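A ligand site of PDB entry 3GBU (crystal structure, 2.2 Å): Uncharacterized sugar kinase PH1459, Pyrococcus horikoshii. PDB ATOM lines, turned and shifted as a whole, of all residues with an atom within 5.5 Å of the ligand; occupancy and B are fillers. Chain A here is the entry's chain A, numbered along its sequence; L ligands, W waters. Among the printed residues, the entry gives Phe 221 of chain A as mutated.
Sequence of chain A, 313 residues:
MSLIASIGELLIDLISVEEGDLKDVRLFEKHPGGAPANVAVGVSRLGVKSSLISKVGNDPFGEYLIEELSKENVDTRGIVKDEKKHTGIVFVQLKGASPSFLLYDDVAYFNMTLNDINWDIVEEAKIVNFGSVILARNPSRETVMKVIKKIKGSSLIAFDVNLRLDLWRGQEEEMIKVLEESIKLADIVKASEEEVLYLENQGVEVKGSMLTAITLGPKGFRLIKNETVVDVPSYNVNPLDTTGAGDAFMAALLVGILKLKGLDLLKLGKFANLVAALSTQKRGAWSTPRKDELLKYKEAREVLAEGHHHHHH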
ATOM      1  N   ASN A 162      -2.603 -12.128 -13.031  1.00  0.00           N
ATOM      2  CA  ASN A 162      -2.415 -12.091 -11.575  1.00  0.00           C
ATOM      3  C   ASN A 162      -2.177 -10.662 -11.035  1.00  0.00           C
ATOM      4  O   ASN A 162      -1.128 -10.354 -10.492  1.00  0.00           O
ATOM      5  CB  ASN A 162      -1.233 -13.015 -11.221  1.00  0.00           C
ATOM      6  CG  ASN A 162      -1.172 -13.346  -9.744  1.00  0.00           C
ATOM      7  OD1 ASN A 162      -2.208 -13.446  -9.073  1.00  0.00           O
ATOM      8  ND2 ASN A 162       0.046 -13.534  -9.215  1.00  0.00           N
ATOM      9  N   ARG A 164      -1.981  -7.436  -8.843  1.00  0.00           N
ATOM     10  CA  ARG A 164      -1.775  -7.071  -7.439  1.00  0.00           C
ATOM     11  C   ARG A 164      -1.464  -5.582  -7.388  1.00  0.00           C
ATOM     12  O   ARG A 164      -0.295  -5.185  -7.346  1.00  0.00           O
ATOM     13  CB  ARG A 164      -0.608  -7.870  -6.835  1.00  0.00           C
ATOM     14  CG  ARG A 164      -0.867  -9.360  -6.754  1.00  0.00           C
ATOM     15  CD  ARG A 164      -1.977  -9.674  -5.773  1.00  0.00           C
ATOM     16  NE  ARG A 164      -2.208 -11.109  -5.690  1.00  0.00           N
ATOM     17  CZ  ARG A 164      -2.802 -11.833  -6.640  1.00  0.00           C
ATOM     18  NH1 ARG A 164      -3.230 -11.265  -7.762  1.00  0.00           N
ATOM     19  NH2 ARG A 164      -2.955 -13.142  -6.463  1.00  0.00           N
ATOM     20  N   LYS A 190      -4.208 -15.863 -19.050  1.00  0.00           N
ATOM     21  CA  LYS A 190      -5.156 -16.265 -18.021  1.00  0.00           C
ATOM     22  C   LYS A 190      -5.506 -15.022 -17.199  1.00  0.00           C
ATOM     23  O   LYS A 190      -4.636 -14.206 -16.913  1.00  0.00           O
ATOM     24  CB  LYS A 190      -4.541 -17.324 -17.097  1.00  0.00           C
ATOM     25  CG  LYS A 190      -5.426 -17.681 -15.885  1.00  0.00           C
ATOM     26  CD  LYS A 190      -4.756 -18.743 -15.008  1.00  0.00           C
ATOM     27  CE  LYS A 190      -5.471 -18.929 -13.671  1.00  0.00           C
ATOM     28  NZ  LYS A 190      -5.360 -17.766 -12.756  1.00  0.00           N
ATOM     29  N   SER A 192      -8.826 -13.276 -14.354  1.00  0.00           N
ATOM     30  CA  SER A 192     -10.135 -13.357 -13.731  1.00  0.00           C
ATOM     31  C   SER A 192     -11.016 -12.337 -14.452  1.00  0.00           C
ATOM     32  O   SER A 192     -10.519 -11.386 -15.054  1.00  0.00           O
ATOM     33  CB  SER A 192     -10.048 -12.997 -12.250  1.00  0.00           C
ATOM     34  OG  SER A 192      -9.822 -11.612 -12.076  1.00  0.00           O
ATOM     35  N   GLU A 195     -10.224  -8.952 -13.475  1.00  0.00           N
ATOM     36  CA  GLU A 195      -9.020  -8.376 -14.064  1.00  0.00           C
ATOM     37  C   GLU A 195      -9.298  -7.940 -15.503  1.00  0.00           C
ATOM     38  O   GLU A 195      -8.783  -6.911 -15.960  1.00  0.00           O
ATOM     39  CB  GLU A 195      -7.868  -9.384 -14.009  1.00  0.00           C
ATOM     40  CG  GLU A 195      -7.512  -9.783 -12.573  1.00  0.00           C
ATOM     41  CD  GLU A 195      -6.527 -10.917 -12.501  1.00  0.00           C
ATOM     42  OE1 GLU A 195      -6.531 -11.765 -13.410  1.00  0.00           O
ATOM     43  OE2 GLU A 195      -5.756 -10.975 -11.515  1.00  0.00           O
ATOM     44  N   THR A 215     -11.331 -16.669 -15.821  1.00  0.00           N
ATOM     45  CA  THR A 215     -11.916 -17.384 -14.687  1.00  0.00           C
ATOM     46  C   THR A 215     -13.051 -16.601 -14.046  1.00  0.00           C
ATOM     47  O   THR A 215     -13.021 -15.369 -13.965  1.00  0.00           O
ATOM     48  CB  THR A 215     -10.829 -17.739 -13.614  1.00  0.00           C
ATOM     49  OG1 THR A 215     -10.233 -16.549 -13.084  1.00  0.00           O
ATOM     50  CG2 THR A 215      -9.757 -18.606 -14.236  1.00  0.00           C
ATOM     51  N   LEU A 216     -14.065 -17.321 -13.615  1.00  0.00           N
ATOM     52  CA  LEU A 216     -15.239 -16.728 -12.990  1.00  0.00           C
ATOM     53  C   LEU A 216     -15.348 -17.217 -11.553  1.00  0.00           C
ATOM     54  O   LEU A 216     -16.424 -17.260 -10.973  1.00  0.00           O
ATOM     55  CB  LEU A 216     -16.483 -17.105 -13.797  1.00  0.00           C
ATOM     56  CG  LEU A 216     -16.344 -16.796 -15.288  1.00  0.00           C
ATOM     57  CD1 LEU A 216     -17.461 -17.468 -16.085  1.00  0.00           C
ATOM     58  CD2 LEU A 216     -16.355 -15.290 -15.476  1.00  0.00           C
ATOM     59  N   GLY A 217     -14.203 -17.601 -10.990  1.00  0.00           N
ATOM     60  CA  GLY A 217     -14.181 -18.088  -9.622  1.00  0.00           C
ATOM     61  C   GLY A 217     -14.870 -19.423  -9.446  1.00  0.00           C
ATOM     62  O   GLY A 217     -14.684 -20.337 -10.248  1.00  0.00           O
ATOM     63  N   PRO A 218     -15.685 -19.560  -8.388  1.00  0.00           N
ATOM     64  CA  PRO A 218     -16.393 -20.808  -8.127  1.00  0.00           C
ATOM     65  C   PRO A 218     -17.426 -21.166  -9.201  1.00  0.00           C
ATOM     66  O   PRO A 218     -17.922 -22.289  -9.229  1.00  0.00           O
ATOM     67  CB  PRO A 218     -17.033 -20.567  -6.752  1.00  0.00           C
ATOM     68  CG  PRO A 218     -17.252 -19.089  -6.745  1.00  0.00           C
ATOM     69  CD  PRO A 218     -15.971 -18.563  -7.338  1.00  0.00           C
ATOM     70  N   GLY A 220     -16.776 -21.350 -12.309  1.00  0.00           N
ATOM     71  CA  GLY A 220     -16.112 -21.990 -13.431  1.00  0.00           C
ATOM     72  C   GLY A 220     -15.268 -21.027 -14.247  1.00  0.00           C
ATOM     73  O   GLY A 220     -14.837 -19.990 -13.752  1.00  0.00           O
ATOM     74  N   PHE A 221     -15.038 -21.363 -15.510  1.00  0.00           N
ATOM     75  CA  PHE A 221     -14.235 -20.526 -16.370  1.00  0.00           C
ATOM     76  C   PHE A 221     -14.710 -20.526 -17.820  1.00  0.00           C
ATOM     77  O   PHE A 221     -15.660 -21.219 -18.181  1.00  0.00           O
ATOM     78  CB  PHE A 221     -12.773 -20.976 -16.308  1.00  0.00           C
ATOM     79  CG  PHE A 221     -12.553 -22.408 -16.697  1.00  0.00           C
ATOM     80  CD1 PHE A 221     -12.156 -22.745 -17.993  1.00  0.00           C
ATOM     81  CD2 PHE A 221     -12.765 -23.433 -15.767  1.00  0.00           C
ATOM     82  CE1 PHE A 221     -11.980 -24.086 -18.351  1.00  0.00           C
ATOM     83  CE2 PHE A 221     -12.588 -24.760 -16.122  1.00  0.00           C
ATOM     84  CZ  PHE A 221     -12.189 -25.083 -17.416  1.00  0.00           C
ATOM     85  N   SER A 234     -18.199 -24.892 -13.236  1.00  0.00           N
ATOM     86  CA  SER A 234     -17.416 -25.612 -12.236  1.00  0.00           C
ATOM     87  C   SER A 234     -17.951 -26.984 -11.900  1.00  0.00           C
ATOM     88  O   SER A 234     -19.164 -27.202 -11.948  1.00  0.00           O
ATOM     89  CB  SER A 234     -17.341 -24.811 -10.934  1.00  0.00           C
ATOM     90  OG  SER A 234     -18.626 -24.632 -10.356  1.00  0.00           O
ATOM     91  N   TYR A 235     -17.053 -27.901 -11.567  1.00  0.00           N
ATOM     92  CA  TYR A 235     -17.445 -29.247 -11.167  1.00  0.00           C
ATOM     93  C   TYR A 235     -18.219 -29.057  -9.878  1.00  0.00           C
ATOM     94  O   TYR A 235     -17.998 -28.089  -9.159  1.00  0.00           O
ATOM     95  CB  TYR A 235     -16.214 -30.116 -10.857  1.00  0.00           C
ATOM     96  CG  TYR A 235     -15.783 -30.995 -11.987  1.00  0.00           C
ATOM     97  CD1 TYR A 235     -16.451 -32.182 -12.273  1.00  0.00           C
ATOM     98  CD2 TYR A 235     -14.708 -30.626 -12.789  1.00  0.00           C
ATOM     99  CE1 TYR A 235     -16.052 -32.990 -13.342  1.00  0.00           C
ATOM    100  CE2 TYR A 235     -14.297 -31.423 -13.848  1.00  0.00           C
ATOM    101  CZ  TYR A 235     -14.969 -32.598 -14.123  1.00  0.00           C
ATOM    102  OH  TYR A 235     -14.533 -33.386 -15.164  1.00  0.00           O
ATOM    103  N   VAL A 237     -18.447 -29.651  -6.423  1.00  0.00           N
ATOM    104  CA  VAL A 237     -17.664 -30.136  -5.293  1.00  0.00           C
ATOM    105  C   VAL A 237     -17.829 -29.232  -4.077  1.00  0.00           C
ATOM    106  O   VAL A 237     -18.271 -28.103  -4.184  1.00  0.00           O
ATOM    107  CB  VAL A 237     -16.134 -30.209  -5.594  1.00  0.00           C
ATOM    108  CG1 VAL A 237     -15.893 -30.888  -6.921  1.00  0.00           C
ATOM    109  CG2 VAL A 237     -15.526 -28.814  -5.598  1.00  0.00           C
ATOM    110  N   PRO A 239     -15.677 -27.385  -1.727  1.00  0.00           N
ATOM    111  CA  PRO A 239     -14.314 -26.877  -1.525  1.00  0.00           C
ATOM    112  C   PRO A 239     -13.788 -26.886  -0.091  1.00  0.00           C
ATOM    113  O   PRO A 239     -14.452 -26.439   0.834  1.00  0.00           O
ATOM    114  CB  PRO A 239     -14.386 -25.450  -2.094  1.00  0.00           C
ATOM    115  CG  PRO A 239     -15.809 -25.069  -1.897  1.00  0.00           C
ATOM    116  CD  PRO A 239     -16.544 -26.332  -2.288  1.00  0.00           C
ATOM    117  N   THR A 242      -9.453 -23.298  -1.527  1.00  0.00           N
ATOM    118  CA  THR A 242      -9.294 -22.858  -2.914  1.00  0.00           C
ATOM    119  C   THR A 242      -8.017 -22.047  -3.154  1.00  0.00           C
ATOM    120  O   THR A 242      -7.789 -21.540  -4.254  1.00  0.00           O
ATOM    121  CB  THR A 242     -10.478 -21.988  -3.362  1.00  0.00           C
ATOM    122  OG1 THR A 242     -10.503 -20.799  -2.559  1.00  0.00           O
ATOM    123  CG2 THR A 242     -11.791 -22.724  -3.160  1.00  0.00           C
ATOM    124  N   ALA A 245      -6.146 -23.276  -6.153  1.00  0.00           N
ATOM    125  CA  ALA A 245      -6.953 -23.572  -7.346  1.00  0.00           C
ATOM    126  C   ALA A 245      -6.499 -22.844  -8.603  1.00  0.00           C
ATOM    127  O   ALA A 245      -6.449 -23.425  -9.681  1.00  0.00           O
ATOM    128  CB  ALA A 245      -8.418 -23.255  -7.064  1.00  0.00           C
ATOM    129  N   GLY A 246      -6.173 -21.567  -8.474  1.00  0.00           N
ATOM    130  CA  GLY A 246      -5.741 -20.798  -9.631  1.00  0.00           C
ATOM    131  C   GLY A 246      -4.502 -21.343 -10.314  1.00  0.00           C
ATOM    132  O   GLY A 246      -4.462 -21.483 -11.533  1.00  0.00           O
ATOM    133  N   ASP A 247      -3.474 -21.646  -9.516  1.00  0.00           N
ATOM    134  CA  ASP A 247      -2.244 -22.153 -10.092  1.00  0.00           C
ATOM    135  C   ASP A 247      -2.382 -23.600 -10.542  1.00  0.00           C
ATOM    136  O   ASP A 247      -1.676 -24.040 -11.450  1.00  0.00           O
ATOM    137  CB  ASP A 247      -1.106 -21.980  -9.081  1.00  0.00           C
ATOM    138  CG  ASP A 247      -0.873 -20.513  -8.734  1.00  0.00           C
ATOM    139  OD1 ASP A 247      -0.982 -19.666  -9.649  1.00  0.00           O
ATOM    140  OD2 ASP A 247      -0.570 -20.205  -7.564  1.00  0.00           O
ATOM    141  N   PHE A 249      -5.158 -24.673 -11.775  1.00  0.00           N
ATOM    142  CA  PHE A 249      -5.860 -24.494 -13.038  1.00  0.00           C
ATOM    143  C   PHE A 249      -4.858 -24.158 -14.161  1.00  0.00           C
ATOM    144  O   PHE A 249      -4.936 -24.739 -15.253  1.00  0.00           O
ATOM    145  CB  PHE A 249      -6.867 -23.353 -12.917  1.00  0.00           C
ATOM    146  CG  PHE A 249      -7.535 -23.004 -14.217  1.00  0.00           C
ATOM    147  CD1 PHE A 249      -8.609 -23.750 -14.694  1.00  0.00           C
ATOM    148  CD2 PHE A 249      -7.111 -21.893 -14.944  1.00  0.00           C
ATOM    149  CE1 PHE A 249      -9.254 -23.389 -15.880  1.00  0.00           C
ATOM    150  CE2 PHE A 249      -7.743 -21.525 -16.134  1.00  0.00           C
ATOM    151  CZ  PHE A 249      -8.824 -22.272 -16.602  1.00  0.00           C
ATOM    152  N   ASN A 273     -10.867 -28.207 -15.569  1.00  0.00           N
ATOM    153  CA  ASN A 273     -11.931 -28.166 -14.570  1.00  0.00           C
ATOM    154  C   ASN A 273     -11.726 -29.266 -13.515  1.00  0.00           C
ATOM    155  O   ASN A 273     -11.816 -29.017 -12.314  1.00  0.00           O
ATOM    156  CB  ASN A 273     -13.298 -28.323 -15.272  1.00  0.00           C
ATOM    157  CG  ASN A 273     -14.453 -27.810 -14.426  1.00  0.00           C
ATOM    158  OD1 ASN A 273     -14.276 -26.934 -13.590  1.00  0.00           O
ATOM    159  ND2 ASN A 273     -15.642 -28.363 -14.661  1.00  0.00           N
ATOM    160  N   ALA A 276      -8.703 -28.425 -11.285  1.00  0.00           N
ATOM    161  CA  ALA A 276      -9.026 -27.315 -10.391  1.00  0.00           C
ATOM    162  C   ALA A 276      -9.943 -27.763  -9.250  1.00  0.00           C
ATOM    163  O   ALA A 276      -9.677 -27.475  -8.071  1.00  0.00           O
ATOM    164  CB  ALA A 276      -9.682 -26.192 -11.177  1.00  0.00           C
ATOM    165  N   ALA A 277     -11.026 -28.454  -9.603  1.00  0.00           N
ATOM    166  CA  ALA A 277     -11.986 -28.935  -8.605  1.00  0.00           C
ATOM    167  C   ALA A 277     -11.306 -29.806  -7.562  1.00  0.00           C
ATOM    168  O   ALA A 277     -11.472 -29.571  -6.367  1.00  0.00           O
ATOM    169  CB  ALA A 277     -13.119 -29.712  -9.307  1.00  0.00           C
ATOM    170  N   THR A 280      -9.155 -28.200  -4.868  1.00  0.00           N
ATOM    171  CA  THR A 280      -9.865 -27.555  -3.753  1.00  0.00           C
ATOM    172  C   THR A 280      -9.964 -28.472  -2.538  1.00  0.00           C
ATOM    173  O   THR A 280     -10.375 -28.039  -1.468  1.00  0.00           O
ATOM    174  CB  THR A 280     -11.296 -27.140  -4.127  1.00  0.00           C
ATOM    175  OG1 THR A 280     -12.071 -28.322  -4.364  1.00  0.00           O
ATOM    176  CG2 THR A 280     -11.300 -26.260  -5.368  1.00  0.00           C
HETATM  177  P1  LIG L   1      -6.784 -15.554  -8.032  1.00  0.00           P
HETATM  178  O1  LIG L   1      -7.525 -14.271  -7.797  1.00  0.00           O
HETATM  179  O2  LIG L   1      -5.295 -15.328  -8.223  1.00  0.00           O
HETATM  180  O3  LIG L   1      -7.089 -16.594  -6.949  1.00  0.00           O
HETATM  181  P2  LIG L   1      -7.807 -17.605  -9.880  1.00  0.00           P
HETATM  182  O4  LIG L   1      -7.726 -17.811 -11.371  1.00  0.00           O
HETATM  183  O5  LIG L   1      -7.026 -18.466  -8.937  1.00  0.00           O
HETATM  184  O6  LIG L   1      -7.386 -16.097  -9.424  1.00  0.00           O
HETATM  185  P3  LIG L   1     -10.144 -18.974  -8.804  1.00  0.00           P
HETATM  186  O7  LIG L   1      -9.315 -19.609  -7.701  1.00  0.00           O
HETATM  187  O8  LIG L   1     -11.540 -18.540  -8.485  1.00  0.00           O
HETATM  188  O9  LIG L   1      -9.368 -17.690  -9.463  1.00  0.00           O
HETATM  189  O10 LIG L   1     -10.185 -19.946 -10.096  1.00  0.00           O
HETATM  190  C1  LIG L   1      -9.390 -21.135 -10.209  1.00  0.00           C
HETATM  191  C2  LIG L   1     -10.288 -22.206 -10.841  1.00  0.00           C
HETATM  192  O11 LIG L   1     -10.466 -23.213  -9.838  1.00  0.00           O
HETATM  193  C3  LIG L   1     -11.709 -21.759 -11.168  1.00  0.00           C
HETATM  194  O12 LIG L   1     -11.847 -21.230 -12.475  1.00  0.00           O
HETATM  195  C4  LIG L   1     -12.522 -22.990 -10.951  1.00  0.00           C
HETATM  196  O13 LIG L   1     -12.638 -23.795 -12.137  1.00  0.00           O
HETATM  197  C5  LIG L   1     -11.805 -23.723  -9.853  1.00  0.00           C
HETATM  198  N1  LIG L   1     -12.559 -23.415  -8.583  1.00  0.00           N
HETATM  199  C6  LIG L   1     -12.392 -22.396  -7.697  1.00  0.00           C
HETATM  200  N2  LIG L   1     -13.284 -22.470  -6.671  1.00  0.00           N
HETATM  201  C7  LIG L   1     -14.039 -23.547  -6.891  1.00  0.00           C
HETATM  202  C8  LIG L   1     -15.174 -24.238  -6.223  1.00  0.00           C
HETATM  203  N3  LIG L   1     -15.675 -23.755  -5.074  1.00  0.00           N
HETATM  204  N4  LIG L   1     -15.686 -25.376  -6.798  1.00  0.00           N
HETATM  205  C9  LIG L   1     -15.194 -25.897  -7.971  1.00  0.00           C
HETATM  206  N5  LIG L   1     -14.166 -25.321  -8.631  1.00  0.00           N
HETATM  207  C10 LIG L   1     -13.565 -24.180  -8.152  1.00  0.00           C
HETATM  208  O   HOH W   1      -7.390 -16.240 -13.332  1.00  0.00           O
HETATM  209  O   HOH W   2     -11.169 -16.268 -10.349  1.00  0.00           O
HETATM  210  O   HOH W   3      -4.451 -15.702 -10.740  1.00  0.00           O
HETATM  211  O   HOH W   4     -10.098 -16.112  -7.638  1.00  0.00           O
HETATM  212  O   HOH W   5      -6.908 -19.765  -6.462  1.00  0.00           O
HETATM  213  O   HOH W   6      -5.376 -12.701  -9.481  1.00  0.00           O
HETATM  214  O   HOH W   7     -10.425 -13.759  -8.129  1.00  0.00           O
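The side-chain hydroxyl (OG) of Ser 234 sits at hydrogen-bond distance from the backbone carbonyl oxygen (O) of Pro 218 (2.7 Å).
The side-chain amide oxygen (OD1) of Asn 162 is in hydrogen-bond range of the guanidinium group (NH2) of Arg 164.
ND2 of Asn 273 lies close to N of Tyr 235 (3.4 Å).
Water W2 lies within hydrogen-bond range of an oxygen (O9) of the ligand (2.5 Å), the side-chain hydroxyl (OG1) of Thr 215 (2.9 Å) and the backbone NH (N) of Gly 217 (3.4 Å).
Water W1 lies within hydrogen-bond range of an oxygen (O4) of the ligand (2.5 Å), the side-chain amino group (NZ) of Lys 190 (2.6 Å), the side-chain hydroxyl (OG1) of Thr 215 (2.9 Å) and the backbone NH (N) of Ser 192 (3.4 Å).
Water W3 lies within hydrogen-bond range of an oxygen (O2) of the ligand (2.7 Å) and the side-chain amino group of Lys 190 (3.0 Å).
Water W5 lies within hydrogen-bond range of O7 of the ligand (2.7 Å), N of Gly 246 (2.8 Å) and O of Thr 242 (3.0 Å).
Water W6 lies within hydrogen-bond range of the side-chain carboxylate of Glu 195, an oxygen (O2) of the ligand, the guanidinium group of Arg 164 and the side-chain amide oxygen of Asn 162.
Asn 162 touches the ligand.
Gly 217 touches the ligand (CA to O8, 2.9 Å).
Pro 218 touches the ligand.
Phe 221 touches the ligand (CD2 to O13, 3.7 Å).
CB of Ser 234 touches C9 of the ligand, at 3.8 Å.
Tyr 235 touches the ligand.
CG2 of Val 237 touches N4 of the ligand (3.6 Å).
Pro 239 touches the ligand.
Thr 242 touches the ligand.
CB of Ala 245 touches O11 of the ligand, at 3.4 Å.
Asn 273 touches the ligand (OD1 to O13, 3.8 Å).
CB of Ala 276 touches O11 of the ligand (3.4 Å).
Hydrophobic or aromatic side chains within 4 Å of the ligand: Pro 218, Phe 221, Val 237, Pro 239, Ala 245 and Ala 276.
Of the 24 residues printed, 17 come within 4 Å of the ligand.
The nearest printed residue that does not touch the ligand is Thr 280 (4.1 Å).
N of Gly 246 sits close to O5 of the ligand.
The guanidinium group of Arg 164 is in salt-bridge range of an oxygen (O2) of the ligand (3.7 Å).
The side-chain hydroxyl (OG1) of Thr 215 is in hydrogen-bond range of an oxygen (O4) of the ligand, at 3.3 Å.
The side-chain amino group (NZ) of Lys 190 lies within salt-bridge range of an oxygen (O4) of the ligand (2.7 Å).
O of Gly 220 sits at hydrogen-bond distance from O12 of the ligand, 3.5 Å away.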
